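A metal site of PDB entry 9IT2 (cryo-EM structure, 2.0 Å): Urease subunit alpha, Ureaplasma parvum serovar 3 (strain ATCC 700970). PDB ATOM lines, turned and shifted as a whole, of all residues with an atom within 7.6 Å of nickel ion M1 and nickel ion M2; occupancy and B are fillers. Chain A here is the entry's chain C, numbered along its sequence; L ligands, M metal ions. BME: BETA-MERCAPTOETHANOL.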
ATOM      1  N   HIS A 141      14.161   8.889 -16.330  1.00  0.00           N
ATOM      2  CA  HIS A 141      14.907   8.314 -15.208  1.00  0.00           C
ATOM      3  C   HIS A 141      16.183   9.134 -15.067  1.00  0.00           C
ATOM      4  O   HIS A 141      17.222   8.789 -15.641  1.00  0.00           O
ATOM      5  CB  HIS A 141      15.204   6.831 -15.439  1.00  0.00           C
ATOM      6  CG  HIS A 141      15.751   6.130 -14.236  1.00  0.00           C
ATOM      7  ND1 HIS A 141      15.641   4.768 -14.053  1.00  0.00           N
ATOM      8  CD2 HIS A 141      16.412   6.601 -13.142  1.00  0.00           C
ATOM      9  CE1 HIS A 141      16.206   4.425 -12.906  1.00  0.00           C
ATOM     10  NE2 HIS A 141      16.683   5.517 -12.337  1.00  0.00           N
ATOM     11  N   VAL A 142      16.112  10.209 -14.298  1.00  0.00           N
ATOM     12  CA  VAL A 142      17.227  11.137 -14.132  1.00  0.00           C
ATOM     13  C   VAL A 142      17.436  11.368 -12.635  1.00  0.00           C
ATOM     14  O   VAL A 142      16.502  11.772 -11.930  1.00  0.00           O
ATOM     15  CB  VAL A 142      16.979  12.475 -14.846  1.00  0.00           C
ATOM     16  CG1 VAL A 142      18.087  13.474 -14.514  1.00  0.00           C
ATOM     17  CG2 VAL A 142      16.876  12.267 -16.345  1.00  0.00           C
ATOM     18  N   HIS A 143      18.646  11.100 -12.159  1.00  0.00           N
ATOM     19  CA  HIS A 143      19.009  11.484 -10.800  1.00  0.00           C
ATOM     20  C   HIS A 143      19.451  12.940 -10.800  1.00  0.00           C
ATOM     21  O   HIS A 143      20.332  13.339 -11.562  1.00  0.00           O
ATOM     22  CB  HIS A 143      20.123  10.583 -10.263  1.00  0.00           C
ATOM     23  CG  HIS A 143      19.703   9.158 -10.061  1.00  0.00           C
ATOM     24  ND1 HIS A 143      19.559   8.584  -8.820  1.00  0.00           N
ATOM     25  CD2 HIS A 143      19.395   8.179 -10.959  1.00  0.00           C
ATOM     26  CE1 HIS A 143      19.181   7.330  -8.952  1.00  0.00           C
ATOM     27  NE2 HIS A 143      19.070   7.055 -10.231  1.00  0.00           N
ATOM     28  N   THR A 172      20.154  10.822  -3.089  1.00  0.00           N
ATOM     29  CA  THR A 172      19.991  11.118  -4.517  1.00  0.00           C
ATOM     30  C   THR A 172      20.915  10.262  -5.359  1.00  0.00           C
ATOM     31  O   THR A 172      20.548   9.839  -6.461  1.00  0.00           O
ATOM     32  CB  THR A 172      20.227  12.599  -4.773  1.00  0.00           C
ATOM     33  OG1 THR A 172      19.242  13.372  -4.070  1.00  0.00           O
ATOM     34  CG2 THR A 172      20.153  12.909  -6.265  1.00  0.00           C
ATOM     35  N   LYS A 173      22.132  10.001  -4.873  1.00  0.00           N
ATOM     36  CA  LYS A 173      23.052   9.140  -5.599  1.00  0.00           C
ATOM     37  C   LYS A 173      22.466   7.740  -5.800  1.00  0.00           C
ATOM     38  O   LYS A 173      22.788   7.067  -6.786  1.00  0.00           O
ATOM     39  CB  LYS A 173      24.390   9.047  -4.866  1.00  0.00           C
ATOM     40  CG  LYS A 173      25.164  10.358  -4.830  1.00  0.00           C
ATOM     41  CD  LYS A 173      26.491  10.204  -4.108  1.00  0.00           C
ATOM     42  CE  LYS A 173      27.143  11.565  -3.869  1.00  0.00           C
ATOM     43  NZ  LYS A 173      28.418  11.448  -3.113  1.00  0.00           N
ATOM     44  N   ALA A 174      21.612   7.293  -4.876  1.00  0.00           N
ATOM     45  CA  ALA A 174      21.012   5.973  -4.972  1.00  0.00           C
ATOM     46  C   ALA A 174      19.663   5.992  -5.696  1.00  0.00           C
ATOM     47  O   ALA A 174      19.394   5.100  -6.513  1.00  0.00           O
ATOM     48  CB  ALA A 174      20.840   5.370  -3.581  1.00  0.00           C
ATOM     49  N   THR A 175      18.814   6.982  -5.418  1.00  0.00           N
ATOM     50  CA  THR A 175      17.437   6.975  -5.875  1.00  0.00           C
ATOM     51  C   THR A 175      17.063   8.306  -6.503  1.00  0.00           C
ATOM     52  O   THR A 175      17.660   9.340  -6.192  1.00  0.00           O
ATOM     53  CB  THR A 175      16.453   6.684  -4.722  1.00  0.00           C
ATOM     54  OG1 THR A 175      16.153   7.910  -4.037  1.00  0.00           O
ATOM     55  CG2 THR A 175      17.055   5.705  -3.722  1.00  0.00           C
ATOM     56  N   THR A 176      16.069   8.282  -7.388  1.00  0.00           N
ATOM     57  CA  THR A 176      15.495   9.490  -7.976  1.00  0.00           C
ATOM     58  C   THR A 176      14.320   9.956  -7.116  1.00  0.00           C
ATOM     59  O   THR A 176      13.144   9.801  -7.471  1.00  0.00           O
ATOM     60  CB  THR A 176      15.062   9.261  -9.411  1.00  0.00           C
ATOM     61  OG1 THR A 176      13.965   8.338  -9.443  1.00  0.00           O
ATOM     62  CG2 THR A 176      16.198   8.687 -10.230  1.00  0.00           C
ATOM     63  N   KCX A 223       8.373   7.912  -6.905  1.00  0.00           N
ATOM     64  CA  KCX A 223       9.329   6.854  -7.185  1.00  0.00           C
ATOM     65  CB  KCX A 223      10.702   7.429  -7.547  1.00  0.00           C
ATOM     66  CG  KCX A 223      11.846   6.421  -7.530  1.00  0.00           C
ATOM     67  CD  KCX A 223      11.760   5.409  -8.666  1.00  0.00           C
ATOM     68  CE  KCX A 223      12.998   4.525  -8.722  1.00  0.00           C
ATOM     69  NZ  KCX A 223      14.253   5.294  -9.000  1.00  0.00           N
ATOM     70  C   KCX A 223       9.455   5.913  -5.991  1.00  0.00           C
ATOM     71  O   KCX A 223       9.741   6.332  -4.878  1.00  0.00           O
ATOM     72  CX  KCX A 223      15.318   4.730  -9.553  1.00  0.00           C
ATOM     73  OQ1 KCX A 223      16.338   5.393  -9.778  1.00  0.00           O
ATOM     74  OQ2 KCX A 223      15.299   3.523  -9.860  1.00  0.00           O
ATOM     75  N   ILE A 224       9.233   4.640  -6.245  1.00  0.00           N
ATOM     76  CA  ILE A 224       9.397   3.621  -5.217  1.00  0.00           C
ATOM     77  C   ILE A 224      10.718   2.896  -5.420  1.00  0.00           C
ATOM     78  O   ILE A 224      10.858   2.089  -6.332  1.00  0.00           O
ATOM     79  CB  ILE A 224       8.228   2.621  -5.214  1.00  0.00           C
ATOM     80  CG1 ILE A 224       6.892   3.359  -5.099  1.00  0.00           C
ATOM     81  CG2 ILE A 224       8.386   1.609  -4.087  1.00  0.00           C
ATOM     82  CD1 ILE A 224       5.695   2.497  -5.408  1.00  0.00           C
ATOM     83  N   HIS A 225      11.692   3.206  -4.564  1.00  0.00           N
ATOM     84  CA  HIS A 225      13.019   2.605  -4.637  1.00  0.00           C
ATOM     85  C   HIS A 225      13.218   1.660  -3.464  1.00  0.00           C
ATOM     86  O   HIS A 225      12.753   1.935  -2.355  1.00  0.00           O
ATOM     87  CB  HIS A 225      14.111   3.680  -4.634  1.00  0.00           C
ATOM     88  CG  HIS A 225      15.352   3.283  -5.349  1.00  0.00           C
ATOM     89  ND1 HIS A 225      16.286   2.420  -4.807  1.00  0.00           N
ATOM     90  CD2 HIS A 225      15.836   3.639  -6.562  1.00  0.00           C
ATOM     91  CE1 HIS A 225      17.280   2.254  -5.669  1.00  0.00           C
ATOM     92  NE2 HIS A 225      17.034   2.979  -6.738  1.00  0.00           N
ATOM     93  N   GLU A 226      13.888   0.537  -3.721  1.00  0.00           N
ATOM     94  CA  GLU A 226      14.127  -0.444  -2.674  1.00  0.00           C
ATOM     95  C   GLU A 226      15.065   0.096  -1.599  1.00  0.00           C
ATOM     96  O   GLU A 226      15.010  -0.349  -0.450  1.00  0.00           O
ATOM     97  CB  GLU A 226      14.690  -1.737  -3.266  1.00  0.00           C
ATOM     98  CG  GLU A 226      16.053  -1.591  -3.919  1.00  0.00           C
ATOM     99  CD  GLU A 226      16.705  -2.918  -4.205  1.00  0.00           C
ATOM    100  OE1 GLU A 226      16.379  -3.904  -3.510  1.00  0.00           O
ATOM    101  OE2 GLU A 226      17.556  -2.982  -5.111  1.00  0.00           O
ATOM    102  N   ILE A 251       8.894   2.554 -10.191  1.00  0.00           N
ATOM    103  CA  ILE A 251       9.303   1.598  -9.164  1.00  0.00           C
ATOM    104  C   ILE A 251      10.702   1.076  -9.462  1.00  0.00           C
ATOM    105  O   ILE A 251      11.051   0.821 -10.620  1.00  0.00           O
ATOM    106  CB  ILE A 251       8.290   0.438  -9.037  1.00  0.00           C
ATOM    107  CG1 ILE A 251       8.691  -0.489  -7.885  1.00  0.00           C
ATOM    108  CG2 ILE A 251       8.155  -0.333 -10.342  1.00  0.00           C
ATOM    109  CD1 ILE A 251       7.517  -1.050  -7.119  1.00  0.00           C
ATOM    110  N   HIS A 252      11.500   0.944  -8.419  1.00  0.00           N
ATOM    111  CA  HIS A 252      12.744   0.191  -8.416  1.00  0.00           C
ATOM    112  C   HIS A 252      12.509  -0.964  -7.445  1.00  0.00           C
ATOM    113  O   HIS A 252      12.668  -0.801  -6.235  1.00  0.00           O
ATOM    114  CB  HIS A 252      13.923   1.078  -8.001  1.00  0.00           C
ATOM    115  CG  HIS A 252      15.243   0.374  -7.988  1.00  0.00           C
ATOM    116  ND1 HIS A 252      16.284   0.726  -8.826  1.00  0.00           N
ATOM    117  CD2 HIS A 252      15.698  -0.658  -7.234  1.00  0.00           C
ATOM    118  CE1 HIS A 252      17.318  -0.056  -8.592  1.00  0.00           C
ATOM    119  NE2 HIS A 252      16.992  -0.911  -7.636  1.00  0.00           N
ATOM    120  N   THR A 253      12.128  -2.121  -7.990  1.00  0.00           N
ATOM    121  CA  THR A 253      11.563  -3.180  -7.171  1.00  0.00           C
ATOM    122  C   THR A 253      12.622  -3.827  -6.278  1.00  0.00           C
ATOM    123  O   THR A 253      13.827  -3.619  -6.440  1.00  0.00           O
ATOM    124  CB  THR A 253      10.895  -4.240  -8.061  1.00  0.00           C
ATOM    125  OG1 THR A 253      11.895  -5.061  -8.663  1.00  0.00           O
ATOM    126  CG2 THR A 253      10.059  -3.585  -9.151  1.00  0.00           C
ATOM    127  N   TYR A 277      10.968   0.903 -13.896  1.00  0.00           N
ATOM    128  CA  TYR A 277      12.302   1.392 -14.182  1.00  0.00           C
ATOM    129  C   TYR A 277      13.267   0.234 -14.401  1.00  0.00           C
ATOM    130  O   TYR A 277      13.278  -0.732 -13.626  1.00  0.00           O
ATOM    131  CB  TYR A 277      12.811   2.269 -13.033  1.00  0.00           C
ATOM    132  CG  TYR A 277      12.478   3.738 -13.155  1.00  0.00           C
ATOM    133  CD1 TYR A 277      11.674   4.202 -14.189  1.00  0.00           C
ATOM    134  CD2 TYR A 277      12.973   4.650 -12.238  1.00  0.00           C
ATOM    135  CE1 TYR A 277      11.378   5.547 -14.295  1.00  0.00           C
ATOM    136  CE2 TYR A 277      12.678   5.995 -12.344  1.00  0.00           C
ATOM    137  CZ  TYR A 277      11.875   6.435 -13.373  1.00  0.00           C
ATOM    138  OH  TYR A 277      11.575   7.771 -13.480  1.00  0.00           O
ATOM    139  N   HIS A 278      14.093   0.341 -15.444  1.00  0.00           N
ATOM    140  CA  HIS A 278      15.140  -0.626 -15.793  1.00  0.00           C
ATOM    141  C   HIS A 278      14.673  -2.060 -15.580  1.00  0.00           C
ATOM    142  O   HIS A 278      15.198  -2.814 -14.764  1.00  0.00           O
ATOM    143  CB  HIS A 278      16.440  -0.347 -15.034  1.00  0.00           C
ATOM    144  CG  HIS A 278      16.273  -0.027 -13.583  1.00  0.00           C
ATOM    145  ND1 HIS A 278      15.531  -0.813 -12.720  1.00  0.00           N
ATOM    146  CD2 HIS A 278      16.748   0.998 -12.838  1.00  0.00           C
ATOM    147  CE1 HIS A 278      15.563  -0.287 -11.514  1.00  0.00           C
ATOM    148  NE2 HIS A 278      16.287   0.817 -11.552  1.00  0.00           N
ATOM    149  N   GLY A 283      20.843  -3.114 -12.831  1.00  0.00           N
ATOM    150  CA  GLY A 283      21.107  -2.217 -11.726  1.00  0.00           C
ATOM    151  C   GLY A 283      20.198  -2.369 -10.532  1.00  0.00           C
ATOM    152  O   GLY A 283      20.494  -1.803  -9.465  1.00  0.00           O
ATOM    153  N   GLY A 284      19.118  -3.125 -10.650  1.00  0.00           N
ATOM    154  CA  GLY A 284      18.196  -3.320  -9.557  1.00  0.00           C
ATOM    155  C   GLY A 284      16.883  -3.917 -10.021  1.00  0.00           C
ATOM    156  O   GLY A 284      16.535  -3.845 -11.202  1.00  0.00           O
ATOM    157  N   GLY A 285      16.142  -4.515  -9.096  1.00  0.00           N
ATOM    158  CA  GLY A 285      14.918  -5.213  -9.448  1.00  0.00           C
ATOM    159  C   GLY A 285      14.943  -6.663  -9.013  1.00  0.00           C
ATOM    160  O   GLY A 285      16.022  -7.219  -8.775  1.00  0.00           O
ATOM    161  N   THR A 304      17.109   1.200 -19.051  1.00  0.00           N
ATOM    162  CA  THR A 304      18.170   2.195 -18.962  1.00  0.00           C
ATOM    163  C   THR A 304      19.277   1.853 -19.946  1.00  0.00           C
ATOM    164  O   THR A 304      19.539   0.688 -20.226  1.00  0.00           O
ATOM    165  CB  THR A 304      18.718   2.284 -17.536  1.00  0.00           C
ATOM    166  OG1 THR A 304      19.152   0.991 -17.108  1.00  0.00           O
ATOM    167  CG2 THR A 304      17.645   2.793 -16.590  1.00  0.00           C
ATOM    168  N   SER A 365      17.772   6.728 -19.065  1.00  0.00           N
ATOM    169  CA  SER A 365      19.206   6.798 -18.822  1.00  0.00           C
ATOM    170  C   SER A 365      19.631   6.287 -17.449  1.00  0.00           C
ATOM    171  O   SER A 365      20.646   5.581 -17.363  1.00  0.00           O
ATOM    172  CB  SER A 365      19.703   8.247 -18.977  1.00  0.00           C
ATOM    173  OG  SER A 365      19.408   9.007 -17.821  1.00  0.00           O
ATOM    174  N   ASP A 366      18.899   6.605 -16.383  1.00  0.00           N
ATOM    175  CA  ASP A 366      19.379   6.462 -15.011  1.00  0.00           C
ATOM    176  C   ASP A 366      20.624   7.328 -14.799  1.00  0.00           C
ATOM    177  O   ASP A 366      21.726   6.848 -14.539  1.00  0.00           O
ATOM    178  CB  ASP A 366      19.662   4.993 -14.652  1.00  0.00           C
ATOM    179  CG  ASP A 366      19.484   4.694 -13.184  1.00  0.00           C
ATOM    180  OD1 ASP A 366      19.273   5.639 -12.392  1.00  0.00           O
ATOM    181  OD2 ASP A 366      19.561   3.504 -12.803  1.00  0.00           O
ATOM    182  N   THR A 367      20.411   8.641 -14.924  1.00  0.00           N
ATOM    183  CA  THR A 367      21.506   9.596 -15.001  1.00  0.00           C
ATOM    184  C   THR A 367      22.395   9.550 -13.773  1.00  0.00           C
ATOM    185  O   THR A 367      21.923   9.668 -12.632  1.00  0.00           O
ATOM    186  CB  THR A 367      20.944  11.008 -15.178  1.00  0.00           C
ATOM    187  OG1 THR A 367      20.267  11.102 -16.443  1.00  0.00           O
ATOM    188  CG2 THR A 367      22.051  12.049 -15.123  1.00  0.00           C
ATOM    189  N   LEU A 368      23.694   9.384 -13.999  1.00  0.00           N
ATOM    190  CA  LEU A 368      24.747   9.482 -12.998  1.00  0.00           C
ATOM    191  C   LEU A 368      24.579   8.516 -11.824  1.00  0.00           C
ATOM    192  O   LEU A 368      25.232   8.690 -10.791  1.00  0.00           O
ATOM    193  CB  LEU A 368      24.883  10.918 -12.473  1.00  0.00           C
ATOM    194  CG  LEU A 368      25.740  11.868 -13.312  1.00  0.00           C
ATOM    195  CD1 LEU A 368      25.536  13.298 -12.864  1.00  0.00           C
ATOM    196  CD2 LEU A 368      27.204  11.481 -13.250  1.00  0.00           C
ATOM    197  N   ALA A 369      23.710   7.513 -11.958  1.00  0.00           N
ATOM    198  CA  ALA A 369      23.644   6.417 -10.998  1.00  0.00           C
ATOM    199  C   ALA A 369      24.019   5.090 -11.631  1.00  0.00           C
ATOM    200  O   ALA A 369      24.792   4.321 -11.046  1.00  0.00           O
ATOM    201  CB  ALA A 369      22.244   6.338 -10.374  1.00  0.00           C
ATOM    202  N   MET A 370      23.484   4.797 -12.817  1.00  0.00           N
ATOM    203  CA  MET A 370      23.956   3.668 -13.614  1.00  0.00           C
ATOM    204  C   MET A 370      24.156   3.989 -15.084  1.00  0.00           C
ATOM    205  O   MET A 370      24.899   3.252 -15.755  1.00  0.00           O
ATOM    206  CB  MET A 370      22.990   2.483 -13.485  1.00  0.00           C
ATOM    207  CG  MET A 370      23.563   1.167 -13.989  1.00  0.00           C
ATOM    208  SD  MET A 370      24.112   0.070 -12.660  1.00  0.00           S
ATOM    209  CE  MET A 370      24.087  -1.506 -13.511  1.00  0.00           C
ATOM    210  N   GLY A 371      23.542   5.034 -15.622  1.00  0.00           N
ATOM    211  CA  GLY A 371      23.615   5.283 -17.051  1.00  0.00           C
ATOM    212  C   GLY A 371      24.000   6.694 -17.448  1.00  0.00           C
ATOM    213  O   GLY A 371      24.411   7.497 -16.606  1.00  0.00           O
HETATM  214  C1  BME L   1      20.424   1.643 -10.210  1.00  0.00           C
HETATM  215  C2  BME L   1      20.408   3.081  -9.685  1.00  0.00           C
HETATM  216  O1  BME L   1      19.369   1.485 -11.139  1.00  0.00           O
HETATM  217  S2  BME L   1      18.705   3.555  -9.313  1.00  0.00           S
HETATM  218 NI    NI M   1      16.703   2.135 -10.144  1.00  0.00          NI
HETATM  219 NI    NI M   2      18.003   5.510 -10.871  1.00  0.00          NI
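O of His 141 lies within hydrogen-bond range of OG of Ser 365 (3.1 Å). A ring nitrogen (NE2) of His 225 lies close to a ring nitrogen (ND1) of His 252 (3.2 Å). O of Ile 224 is in hydrogen-bond range of N of His 252 (2.5 Å). O of His 252 is in hydrogen-bond range of N of Glu 226 (3.1 Å). O of Thr 172 is in hydrogen-bond range of ND1 of His 143 (2.8 Å). The backbone carbonyl oxygen (O) of Asp 366 lies within hydrogen-bond range of the backbone NH (N) of Gly 371 (2.8 Å). The side-chain hydroxyl of Thr 176 sits at hydrogen-bond distance from NZ of KCX 223 (3.1 Å). A ring nitrogen (NE2) of His 225 is in hydrogen-bond range of the backbone carbonyl oxygen of Ala 174 (3.2 Å).
Merely in contact with nickel ion M1: His 225.
CG2 of Thr 176 touches nickel ion M2, 3.7 Å away. Within 4 Å of nickel ion M2: His 141, His 143, Thr 176, KCX 223 and Asp 366. The nearest printed residue that does not touch nickel ion M2 is Ala 369 (4.3 Å).
Nickel ion M1 is bound by NE2 of His 278. Nickel ion M1 is bound by ND1 of His 252, 2.0 Å away. OQ2 of KCX 223 binds nickel ion M1 (2.0 Å). A sulfur (S2) of the ligand is bound to nickel ion M1, at 2.6 Å. Nickel ion M1 has four donor atoms within binding distance.
NE2 of His 141 is bound to nickel ion M2 (2.0 Å). Nickel ion M2 is bound by a ring nitrogen (NE2) of His 143 (2.0 Å). Nickel ion M2 is bound by OD1 of Asp 366, 2.0 Å away. Nickel ion M2 is bound by OQ1 of KCX 223 (2.0 Å). Nickel ion M2 is bound by S2 of the ligand. Nickel ion M2 has five donor atoms within binding distance.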
